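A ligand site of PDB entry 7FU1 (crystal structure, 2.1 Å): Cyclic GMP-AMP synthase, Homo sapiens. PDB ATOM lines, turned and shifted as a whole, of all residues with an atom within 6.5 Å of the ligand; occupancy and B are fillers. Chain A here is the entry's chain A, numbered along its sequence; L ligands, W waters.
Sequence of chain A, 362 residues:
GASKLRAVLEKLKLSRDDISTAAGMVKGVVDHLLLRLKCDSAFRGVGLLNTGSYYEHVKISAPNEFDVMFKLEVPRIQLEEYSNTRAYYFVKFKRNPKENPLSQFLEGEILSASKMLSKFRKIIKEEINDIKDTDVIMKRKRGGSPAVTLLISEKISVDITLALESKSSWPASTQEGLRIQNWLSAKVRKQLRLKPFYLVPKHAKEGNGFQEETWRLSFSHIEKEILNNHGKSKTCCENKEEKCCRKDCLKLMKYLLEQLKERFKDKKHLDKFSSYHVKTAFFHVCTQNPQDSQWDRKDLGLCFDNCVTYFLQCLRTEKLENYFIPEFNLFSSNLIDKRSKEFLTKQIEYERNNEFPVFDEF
The side-chain amide nitrogen (ND2) of Asn 322 is in hydrogen-bond range of an oxygen (O1) of the ligand, 2.6 Å away. The side-chain hydroxyl (OG) of Ser 274 lies within hydrogen-bond range of an oxygen (O3) of the ligand (2.9 Å). N of Phe 219 lies within hydrogen-bond range of O4 of the ligand (2.9 Å). The backbone carbonyl oxygen of Leu 217 lies close to a nitrogen (N1) of the ligand (3.5 Å).
ND2 of Asn 322 lies within hydrogen-bond range of OH of Tyr 276 (3.3 Å). The backbone NH (N) of Phe 324 lies within hydrogen-bond range of the side-chain amide oxygen (OD1) of Asn 322 (2.7 Å). N of Asn 322 sits at hydrogen-bond distance from O of Phe 328 (2.8 Å). N of Ile 325 lies within hydrogen-bond range of OD1 of Asn 322. A ring nitrogen (ND1) of His 277 is in hydrogen-bond range of the backbone NH (N) of Ser 274. The backbone carbonyl oxygen of Tyr 276 is in hydrogen-bond range of the side-chain hydroxyl of Thr 280 (2.8 Å). The side-chain carboxylate of Glu 223 is in salt-bridge range of the side-chain amino group of Lys 279 (3.2 Å). The backbone carbonyl oxygen of Phe 283 lies within hydrogen-bond range of the side-chain hydroxyl of Tyr 323.
Ala 87 touches the ligand. Tyr 88 touches the ligand. NZ of Lys 202 touches C7 of the ligand, 3.4 Å away. NH1 of Arg 216 touches C10 of the ligand, 3.0 Å away. Ser 218 touches the ligand (CA to O4, 3.6 Å). Ser 220 touches the ligand. OE1 of Glu 223 touches C18 of the ligand (3.2 Å). CE2 of Tyr 276 touches N2 of the ligand, at 3.1 Å. Lys 279 touches the ligand. CE2 of Phe 283 touches BR1 of the ligand, 3.4 Å away. Phe 324 touches the ligand (CE1 to C1, 3.6 Å). Phe 328 touches the ligand (CE2 to C3, 3.98 Å). Hydrophobic or aromatic side chains that line the ligand: Ala 87, Phe 219, Tyr 276, Phe 283, Phe 324 and Phe 328.
Water W1 lies within hydrogen-bond range of the side-chain hydroxyl of Thr 280 (2.8 Å), an oxygen (O1) of the ligand (2.8 Å), the backbone NH of Tyr 323 (2.9 Å) and the side-chain amide nitrogen of Asn 322 (3.3 Å).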
ATOM      1  N   ALA A  87     -22.505 -19.093 -20.942  1.00  0.00           N
ATOM      2  CA  ALA A  87     -22.335 -20.361 -20.234  1.00  0.00           C
ATOM      3  C   ALA A  87     -21.491 -20.290 -18.970  1.00  0.00           C
ATOM      4  O   ALA A  87     -21.517 -21.247 -18.191  1.00  0.00           O
ATOM      5  CB  ALA A  87     -21.696 -21.416 -21.150  1.00  0.00           C
ATOM      6  N   TYR A  88     -20.741 -19.231 -18.759  1.00  0.00           N
ATOM      7  CA  TYR A  88     -19.826 -19.130 -17.627  1.00  0.00           C
ATOM      8  C   TYR A  88     -20.286 -18.005 -16.707  1.00  0.00           C
ATOM      9  O   TYR A  88     -20.777 -16.967 -17.177  1.00  0.00           O
ATOM     10  CB  TYR A  88     -18.384 -18.919 -18.140  1.00  0.00           C
ATOM     11  CG  TYR A  88     -17.788 -20.130 -18.891  1.00  0.00           C
ATOM     12  CD1 TYR A  88     -17.180 -21.165 -18.179  1.00  0.00           C
ATOM     13  CD2 TYR A  88     -17.811 -20.218 -20.281  1.00  0.00           C
ATOM     14  CE1 TYR A  88     -16.627 -22.268 -18.826  1.00  0.00           C
ATOM     15  CE2 TYR A  88     -17.242 -21.329 -20.950  1.00  0.00           C
ATOM     16  CZ  TYR A  88     -16.657 -22.353 -20.205  1.00  0.00           C
ATOM     17  OH  TYR A  88     -16.093 -23.477 -20.784  1.00  0.00           O
ATOM     18  N   LYS A 202     -14.518 -23.991 -14.257  1.00  0.00           N
ATOM     19  CA  LYS A 202     -13.791 -24.049 -15.529  1.00  0.00           C
ATOM     20  C   LYS A 202     -13.634 -22.634 -16.084  1.00  0.00           C
ATOM     21  O   LYS A 202     -14.278 -21.710 -15.576  1.00  0.00           O
ATOM     22  CB  LYS A 202     -14.489 -24.946 -16.573  1.00  0.00           C
ATOM     23  CG  LYS A 202     -13.538 -25.474 -17.690  1.00  0.00           C
ATOM     24  CD  LYS A 202     -14.254 -25.904 -18.985  1.00  0.00           C
ATOM     25  CE  LYS A 202     -13.276 -25.923 -20.183  1.00  0.00           C
ATOM     26  NZ  LYS A 202     -13.569 -26.930 -21.247  1.00  0.00           N
ATOM     27  N   ARG A 216     -19.501 -23.088 -14.454  1.00  0.00           N
ATOM     28  CA  ARG A 216     -20.153 -23.509 -15.680  1.00  0.00           C
ATOM     29  C   ARG A 216     -21.294 -24.468 -15.347  1.00  0.00           C
ATOM     30  O   ARG A 216     -21.195 -25.262 -14.411  1.00  0.00           O
ATOM     31  CB  ARG A 216     -19.133 -24.161 -16.591  1.00  0.00           C
ATOM     32  CG  ARG A 216     -19.631 -24.559 -17.932  1.00  0.00           C
ATOM     33  CD  ARG A 216     -18.820 -25.745 -18.361  1.00  0.00           C
ATOM     34  NE  ARG A 216     -19.353 -26.973 -17.773  1.00  0.00           N
ATOM     35  CZ  ARG A 216     -18.775 -28.157 -17.918  1.00  0.00           C
ATOM     36  NH1 ARG A 216     -17.637 -28.268 -18.608  1.00  0.00           N
ATOM     37  NH2 ARG A 216     -19.334 -29.230 -17.374  1.00  0.00           N
ATOM     38  N   LEU A 217     -22.370 -24.376 -16.121  1.00  0.00           N
ATOM     39  CA  LEU A 217     -23.531 -25.232 -15.892  1.00  0.00           C
ATOM     40  C   LEU A 217     -23.221 -26.681 -16.259  1.00  0.00           C
ATOM     41  O   LEU A 217     -22.554 -26.966 -17.264  1.00  0.00           O
ATOM     42  CB  LEU A 217     -24.698 -24.738 -16.730  1.00  0.00           C
ATOM     43  CG  LEU A 217     -25.554 -23.587 -16.248  1.00  0.00           C
ATOM     44  CD1 LEU A 217     -26.162 -22.831 -17.438  1.00  0.00           C
ATOM     45  CD2 LEU A 217     -26.637 -24.179 -15.391  1.00  0.00           C
ATOM     46  N   SER A 218     -23.750 -27.608 -15.457  1.00  0.00           N
ATOM     47  CA  SER A 218     -23.591 -29.042 -15.658  1.00  0.00           C
ATOM     48  C   SER A 218     -24.968 -29.691 -15.748  1.00  0.00           C
ATOM     49  O   SER A 218     -25.841 -29.396 -14.927  1.00  0.00           O
ATOM     50  CB  SER A 218     -22.767 -29.664 -14.525  1.00  0.00           C
ATOM     51  OG  SER A 218     -22.678 -31.080 -14.674  1.00  0.00           O
ATOM     52  N   PHE A 219     -25.158 -30.548 -16.764  1.00  0.00           N
ATOM     53  CA  PHE A 219     -26.463 -31.141 -17.036  1.00  0.00           C
ATOM     54  C   PHE A 219     -26.413 -32.662 -17.187  1.00  0.00           C
ATOM     55  O   PHE A 219     -27.295 -33.244 -17.821  1.00  0.00           O
ATOM     56  CB  PHE A 219     -27.080 -30.540 -18.315  1.00  0.00           C
ATOM     57  CG  PHE A 219     -27.497 -29.118 -18.173  1.00  0.00           C
ATOM     58  CD1 PHE A 219     -28.687 -28.809 -17.524  1.00  0.00           C
ATOM     59  CD2 PHE A 219     -26.723 -28.095 -18.693  1.00  0.00           C
ATOM     60  CE1 PHE A 219     -29.109 -27.480 -17.373  1.00  0.00           C
ATOM     61  CE2 PHE A 219     -27.141 -26.757 -18.578  1.00  0.00           C
ATOM     62  CZ  PHE A 219     -28.335 -26.447 -17.897  1.00  0.00           C
ATOM     63  N   SER A 220     -25.386 -33.319 -16.642  1.00  0.00           N
ATOM     64  CA  SER A 220     -25.249 -34.768 -16.791  1.00  0.00           C
ATOM     65  C   SER A 220     -26.454 -35.510 -16.246  1.00  0.00           C
ATOM     66  O   SER A 220     -26.728 -36.637 -16.666  1.00  0.00           O
ATOM     67  CB  SER A 220     -23.985 -35.265 -16.090  1.00  0.00           C
ATOM     68  OG  SER A 220     -22.811 -34.970 -16.819  1.00  0.00           O
ATOM     69  N   HIS A 221     -27.164 -34.932 -15.281  1.00  0.00           N
ATOM     70  CA  HIS A 221     -28.331 -35.598 -14.726  1.00  0.00           C
ATOM     71  C   HIS A 221     -29.524 -35.540 -15.677  1.00  0.00           C
ATOM     72  O   HIS A 221     -30.372 -36.440 -15.661  1.00  0.00           O
ATOM     73  CB  HIS A 221     -28.712 -34.989 -13.381  1.00  0.00           C
ATOM     74  CG  HIS A 221     -29.011 -33.523 -13.449  1.00  0.00           C
ATOM     75  ND1 HIS A 221     -28.146 -32.615 -14.028  1.00  0.00           N
ATOM     76  CD2 HIS A 221     -30.058 -32.803 -12.983  1.00  0.00           C
ATOM     77  CE1 HIS A 221     -28.663 -31.401 -13.948  1.00  0.00           C
ATOM     78  NE2 HIS A 221     -29.826 -31.484 -13.310  1.00  0.00           N
ATOM     79  N   GLU A 223     -29.195 -35.403 -19.055  1.00  0.00           N
ATOM     80  CA  GLU A 223     -28.758 -36.384 -20.048  1.00  0.00           C
ATOM     81  C   GLU A 223     -29.127 -37.808 -19.636  1.00  0.00           C
ATOM     82  O   GLU A 223     -29.813 -38.521 -20.367  1.00  0.00           O
ATOM     83  CB  GLU A 223     -27.254 -36.252 -20.250  1.00  0.00           C
ATOM     84  CG  GLU A 223     -26.617 -37.319 -21.172  1.00  0.00           C
ATOM     85  CD  GLU A 223     -25.144 -37.531 -20.841  1.00  0.00           C
ATOM     86  OE1 GLU A 223     -24.485 -36.561 -20.422  1.00  0.00           O
ATOM     87  OE2 GLU A 223     -24.661 -38.676 -20.968  1.00  0.00           O
ATOM     88  N   LYS A 272      -9.055 -31.085 -28.067  1.00  0.00           N
ATOM     89  CA  LYS A 272     -10.148 -30.285 -27.552  1.00  0.00           C
ATOM     90  C   LYS A 272     -11.513 -30.946 -27.683  1.00  0.00           C
ATOM     91  O   LYS A 272     -12.464 -30.518 -27.005  1.00  0.00           O
ATOM     92  CB  LYS A 272     -10.164 -28.906 -28.198  1.00  0.00           C
ATOM     93  CG  LYS A 272      -8.876 -28.124 -27.993  1.00  0.00           C
ATOM     94  CD  LYS A 272      -9.086 -26.657 -28.347  1.00  0.00           C
ATOM     95  CE  LYS A 272      -7.772 -25.903 -28.588  1.00  0.00           C
ATOM     96  NZ  LYS A 272      -7.853 -24.947 -29.772  1.00  0.00           N
ATOM     97  N   PHE A 273     -11.663 -31.977 -28.513  1.00  0.00           N
ATOM     98  CA  PHE A 273     -12.951 -32.667 -28.598  1.00  0.00           C
ATOM     99  C   PHE A 273     -13.097 -33.718 -27.496  1.00  0.00           C
ATOM    100  O   PHE A 273     -12.122 -34.342 -27.078  1.00  0.00           O
ATOM    101  CB  PHE A 273     -13.118 -33.369 -29.945  1.00  0.00           C
ATOM    102  CG  PHE A 273     -12.941 -32.467 -31.146  1.00  0.00           C
ATOM    103  CD1 PHE A 273     -13.981 -31.676 -31.603  1.00  0.00           C
ATOM    104  CD2 PHE A 273     -11.746 -32.459 -31.853  1.00  0.00           C
ATOM    105  CE1 PHE A 273     -13.828 -30.873 -32.724  1.00  0.00           C
ATOM    106  CE2 PHE A 273     -11.592 -31.657 -32.975  1.00  0.00           C
ATOM    107  CZ  PHE A 273     -12.629 -30.859 -33.412  1.00  0.00           C
ATOM    108  N   SER A 274     -14.342 -33.939 -27.064  1.00  0.00           N
ATOM    109  CA  SER A 274     -14.679 -34.913 -26.031  1.00  0.00           C
ATOM    110  C   SER A 274     -16.083 -35.482 -26.301  1.00  0.00           C
ATOM    111  O   SER A 274     -16.770 -35.047 -27.223  1.00  0.00           O
ATOM    112  CB  SER A 274     -14.633 -34.289 -24.644  1.00  0.00           C
ATOM    113  OG  SER A 274     -15.611 -33.287 -24.538  1.00  0.00           O
ATOM    114  N   SER A 275     -16.497 -36.435 -25.473  1.00  0.00           N
ATOM    115  CA  SER A 275     -17.816 -37.040 -25.653  1.00  0.00           C
ATOM    116  C   SER A 275     -18.942 -36.016 -25.522  1.00  0.00           C
ATOM    117  O   SER A 275     -20.069 -36.245 -25.991  1.00  0.00           O
ATOM    118  CB  SER A 275     -17.977 -38.181 -24.637  1.00  0.00           C
ATOM    119  OG  SER A 275     -18.438 -37.660 -23.408  1.00  0.00           O
ATOM    120  N   TYR A 276     -18.670 -34.868 -24.905  1.00  0.00           N
ATOM    121  CA  TYR A 276     -19.655 -33.805 -24.806  1.00  0.00           C
ATOM    122  C   TYR A 276     -20.023 -33.275 -26.191  1.00  0.00           C
ATOM    123  O   TYR A 276     -21.203 -33.031 -26.498  1.00  0.00           O
ATOM    124  CB  TYR A 276     -19.087 -32.715 -23.892  1.00  0.00           C
ATOM    125  CG  TYR A 276     -19.516 -31.285 -24.145  1.00  0.00           C
ATOM    126  CD1 TYR A 276     -20.802 -30.858 -23.792  1.00  0.00           C
ATOM    127  CD2 TYR A 276     -18.620 -30.339 -24.636  1.00  0.00           C
ATOM    128  CE1 TYR A 276     -21.198 -29.525 -23.990  1.00  0.00           C
ATOM    129  CE2 TYR A 276     -19.006 -29.007 -24.835  1.00  0.00           C
ATOM    130  CZ  TYR A 276     -20.289 -28.609 -24.506  1.00  0.00           C
ATOM    131  OH  TYR A 276     -20.671 -27.291 -24.680  1.00  0.00           O
ATOM    132  N   HIS A 277     -19.037 -33.083 -27.061  1.00  0.00           N
ATOM    133  CA  HIS A 277     -19.328 -32.664 -28.426  1.00  0.00           C
ATOM    134  C   HIS A 277     -20.165 -33.700 -29.162  1.00  0.00           C
ATOM    135  O   HIS A 277     -20.962 -33.352 -30.033  1.00  0.00           O
ATOM    136  CB  HIS A 277     -18.016 -32.406 -29.163  1.00  0.00           C
ATOM    137  CG  HIS A 277     -17.188 -31.324 -28.547  1.00  0.00           C
ATOM    138  ND1 HIS A 277     -16.234 -31.574 -27.590  1.00  0.00           N
ATOM    139  CD2 HIS A 277     -17.226 -29.984 -28.695  1.00  0.00           C
ATOM    140  CE1 HIS A 277     -15.688 -30.432 -27.201  1.00  0.00           C
ATOM    141  NE2 HIS A 277     -16.270 -29.453 -27.857  1.00  0.00           N
ATOM    142  N   LYS A 279     -22.228 -36.175 -27.629  1.00  0.00           N
ATOM    143  CA  LYS A 279     -23.557 -36.152 -26.999  1.00  0.00           C
ATOM    144  C   LYS A 279     -24.414 -35.036 -27.544  1.00  0.00           C
ATOM    145  O   LYS A 279     -25.568 -35.245 -27.949  1.00  0.00           O
ATOM    146  CB  LYS A 279     -23.406 -35.999 -25.496  1.00  0.00           C
ATOM    147  CG  LYS A 279     -22.789 -37.162 -24.789  1.00  0.00           C
ATOM    148  CD  LYS A 279     -22.623 -36.784 -23.306  1.00  0.00           C
ATOM    149  CE  LYS A 279     -21.938 -37.862 -22.491  1.00  0.00           C
ATOM    150  NZ  LYS A 279     -21.494 -37.288 -21.194  1.00  0.00           N
ATOM    151  N   THR A 280     -23.861 -33.823 -27.585  1.00  0.00           N
ATOM    152  CA  THR A 280     -24.610 -32.653 -28.020  1.00  0.00           C
ATOM    153  C   THR A 280     -25.125 -32.833 -29.437  1.00  0.00           C
ATOM    154  O   THR A 280     -26.310 -32.599 -29.708  1.00  0.00           O
ATOM    155  CB  THR A 280     -23.722 -31.408 -27.972  1.00  0.00           C
ATOM    156  OG1 THR A 280     -23.347 -31.161 -26.621  1.00  0.00           O
ATOM    157  CG2 THR A 280     -24.496 -30.194 -28.501  1.00  0.00           C
ATOM    158  N   PHE A 283     -28.050 -35.452 -29.559  1.00  0.00           N
ATOM    159  CA  PHE A 283     -29.384 -35.012 -29.135  1.00  0.00           C
ATOM    160  C   PHE A 283     -30.001 -34.081 -30.175  1.00  0.00           C
ATOM    161  O   PHE A 283     -31.230 -34.066 -30.314  1.00  0.00           O
ATOM    162  CB  PHE A 283     -29.327 -34.342 -27.764  1.00  0.00           C
ATOM    163  CG  PHE A 283     -29.111 -35.302 -26.618  1.00  0.00           C
ATOM    164  CD1 PHE A 283     -29.810 -36.494 -26.553  1.00  0.00           C
ATOM    165  CD2 PHE A 283     -28.187 -35.024 -25.619  1.00  0.00           C
ATOM    166  CE1 PHE A 283     -29.614 -37.396 -25.485  1.00  0.00           C
ATOM    167  CE2 PHE A 283     -27.981 -35.926 -24.554  1.00  0.00           C
ATOM    168  CZ  PHE A 283     -28.697 -37.094 -24.481  1.00  0.00           C
ATOM    169  N   ASN A 322     -24.668 -25.611 -28.244  1.00  0.00           N
ATOM    170  CA  ASN A 322     -24.949 -26.283 -26.987  1.00  0.00           C
ATOM    171  C   ASN A 322     -26.425 -26.609 -26.933  1.00  0.00           C
ATOM    172  O   ASN A 322     -27.255 -25.804 -27.364  1.00  0.00           O
ATOM    173  CB  ASN A 322     -24.541 -25.388 -25.805  1.00  0.00           C
ATOM    174  CG  ASN A 322     -24.808 -26.067 -24.474  1.00  0.00           C
ATOM    175  OD1 ASN A 322     -25.945 -26.158 -24.021  1.00  0.00           O
ATOM    176  ND2 ASN A 322     -23.762 -26.562 -23.845  1.00  0.00           N
ATOM    177  N   TYR A 323     -26.748 -27.807 -26.432  1.00  0.00           N
ATOM    178  CA  TYR A 323     -28.109 -28.330 -26.490  1.00  0.00           C
ATOM    179  C   TYR A 323     -29.003 -27.689 -25.442  1.00  0.00           C
ATOM    180  O   TYR A 323     -30.244 -27.796 -25.539  1.00  0.00           O
ATOM    181  CB  TYR A 323     -28.100 -29.867 -26.305  1.00  0.00           C
ATOM    182  CG  TYR A 323     -29.396 -30.537 -26.716  1.00  0.00           C
ATOM    183  CD1 TYR A 323     -29.800 -30.556 -28.047  1.00  0.00           C
ATOM    184  CD2 TYR A 323     -30.250 -31.130 -25.779  1.00  0.00           C
ATOM    185  CE1 TYR A 323     -30.984 -31.139 -28.445  1.00  0.00           C
ATOM    186  CE2 TYR A 323     -31.449 -31.747 -26.184  1.00  0.00           C
ATOM    187  CZ  TYR A 323     -31.799 -31.726 -27.518  1.00  0.00           C
ATOM    188  OH  TYR A 323     -32.979 -32.310 -27.949  1.00  0.00           O
ATOM    189  N   PHE A 324     -28.406 -27.056 -24.443  1.00  0.00           N
ATOM    190  CA  PHE A 324     -29.127 -26.414 -23.346  1.00  0.00           C
ATOM    191  C   PHE A 324     -29.076 -24.904 -23.417  1.00  0.00           C
ATOM    192  O   PHE A 324     -29.948 -24.234 -22.865  1.00  0.00           O
ATOM    193  CB  PHE A 324     -28.555 -26.857 -22.001  1.00  0.00           C
ATOM    194  CG  PHE A 324     -28.792 -28.289 -21.701  1.00  0.00           C
ATOM    195  CD1 PHE A 324     -27.970 -29.253 -22.225  1.00  0.00           C
ATOM    196  CD2 PHE A 324     -29.849 -28.671 -20.906  1.00  0.00           C
ATOM    197  CE1 PHE A 324     -28.189 -30.607 -21.974  1.00  0.00           C
ATOM    198  CE2 PHE A 324     -30.070 -30.027 -20.665  1.00  0.00           C
ATOM    199  CZ  PHE A 324     -29.228 -30.984 -21.195  1.00  0.00           C
ATOM    200  N   ILE A 325     -28.077 -24.359 -24.102  1.00  0.00           N
ATOM    201  CA  ILE A 325     -27.775 -22.938 -24.103  1.00  0.00           C
ATOM    202  C   ILE A 325     -27.509 -22.584 -25.566  1.00  0.00           C
ATOM    203  O   ILE A 325     -26.356 -22.672 -26.020  1.00  0.00           O
ATOM    204  CB  ILE A 325     -26.545 -22.624 -23.233  1.00  0.00           C
ATOM    205  CG1 ILE A 325     -26.735 -23.184 -21.817  1.00  0.00           C
ATOM    206  CG2 ILE A 325     -26.290 -21.116 -23.197  1.00  0.00           C
ATOM    207  CD1 ILE A 325     -25.413 -23.429 -21.080  1.00  0.00           C
ATOM    208  N   PHE A 328     -24.462 -20.647 -27.492  1.00  0.00           N
ATOM    209  CA  PHE A 328     -23.103 -21.071 -27.242  1.00  0.00           C
ATOM    210  C   PHE A 328     -22.715 -22.087 -28.319  1.00  0.00           C
ATOM    211  O   PHE A 328     -23.319 -23.160 -28.397  1.00  0.00           O
ATOM    212  CB  PHE A 328     -22.993 -21.675 -25.843  1.00  0.00           C
ATOM    213  CG  PHE A 328     -21.588 -22.017 -25.435  1.00  0.00           C
ATOM    214  CD1 PHE A 328     -20.755 -21.056 -24.900  1.00  0.00           C
ATOM    215  CD2 PHE A 328     -21.112 -23.297 -25.592  1.00  0.00           C
ATOM    216  CE1 PHE A 328     -19.476 -21.375 -24.526  1.00  0.00           C
ATOM    217  CE2 PHE A 328     -19.814 -23.618 -25.222  1.00  0.00           C
ATOM    218  CZ  PHE A 328     -19.002 -22.658 -24.693  1.00  0.00           C
ATOM    219  N   LEU A 330     -20.184 -24.613 -29.655  1.00  0.00           N
ATOM    220  CA  LEU A 330     -19.083 -25.467 -29.224  1.00  0.00           C
ATOM    221  C   LEU A 330     -17.951 -25.455 -30.218  1.00  0.00           C
ATOM    222  O   LEU A 330     -16.791 -25.612 -29.838  1.00  0.00           O
ATOM    223  CB  LEU A 330     -19.535 -26.918 -29.033  1.00  0.00           C
ATOM    224  CG  LEU A 330     -20.362 -27.309 -27.823  1.00  0.00           C
ATOM    225  CD1 LEU A 330     -21.517 -26.365 -27.650  1.00  0.00           C
ATOM    226  CD2 LEU A 330     -20.902 -28.694 -28.019  1.00  0.00           C
HETATM  227  C1  LIG L   1     -24.631 -31.376 -22.148  1.00  0.00           C
HETATM  228  C2  LIG L   1     -21.592 -26.685 -20.865  1.00  0.00           C
HETATM  229  C3  LIG L   1     -20.104 -24.893 -21.460  1.00  0.00           C
HETATM  230  C4  LIG L   1     -19.092 -25.802 -21.699  1.00  0.00           C
HETATM  231  C5  LIG L   1     -19.299 -27.151 -21.496  1.00  0.00           C
HETATM  232  C6  LIG L   1     -18.225 -28.132 -21.758  1.00  0.00           C
HETATM  233  C7  LIG L   1     -15.207 -28.811 -23.492  1.00  0.00           C
HETATM  234  C8  LIG L   1     -16.896 -29.906 -21.887  1.00  0.00           C
HETATM  235  C9  LIG L   1     -16.255 -31.220 -21.747  1.00  0.00           C
HETATM  236  C10 LIG L   1     -18.067 -29.442 -21.313  1.00  0.00           C
HETATM  237  C11 LIG L   1     -20.567 -27.601 -21.094  1.00  0.00           C
HETATM  238  C12 LIG L   1     -22.982 -27.107 -20.414  1.00  0.00           C
HETATM  239  C13 LIG L   1     -21.349 -25.330 -21.046  1.00  0.00           C
HETATM  240  C14 LIG L   1     -23.821 -29.218 -21.291  1.00  0.00           C
HETATM  241  C15 LIG L   1     -24.039 -30.682 -21.091  1.00  0.00           C
HETATM  242  C16 LIG L   1     -23.711 -31.370 -19.906  1.00  0.00           C
HETATM  243  C17 LIG L   1     -23.971 -32.742 -19.812  1.00  0.00           C
HETATM  244  C18 LIG L   1     -24.543 -33.427 -20.876  1.00  0.00           C
HETATM  245  C19 LIG L   1     -24.863 -32.728 -22.024  1.00  0.00           C
HETATM  246  N1  LIG L   1     -23.233 -28.536 -20.304  1.00  0.00           N
HETATM  247  N2  LIG L   1     -17.219 -27.774 -22.599  1.00  0.00           N
HETATM  248  N3  LIG L   1     -16.413 -28.863 -22.662  1.00  0.00           N
HETATM  249  O1  LIG L   1     -24.159 -28.679 -22.352  1.00  0.00           O
HETATM  250  O2  LIG L   1     -16.932 -32.028 -20.973  1.00  0.00           O
HETATM  251  O3  LIG L   1     -15.200 -31.538 -22.300  1.00  0.00           O
HETATM  252  O4  LIG L   1     -23.163 -30.718 -18.848  1.00  0.00           O
HETATM  253 BR1  LIG L   1     -25.651 -33.650 -23.480  1.00  0.00          BR
HETATM  254  O   HOH W   1     -24.797 -29.429 -24.997  1.00  0.00           O
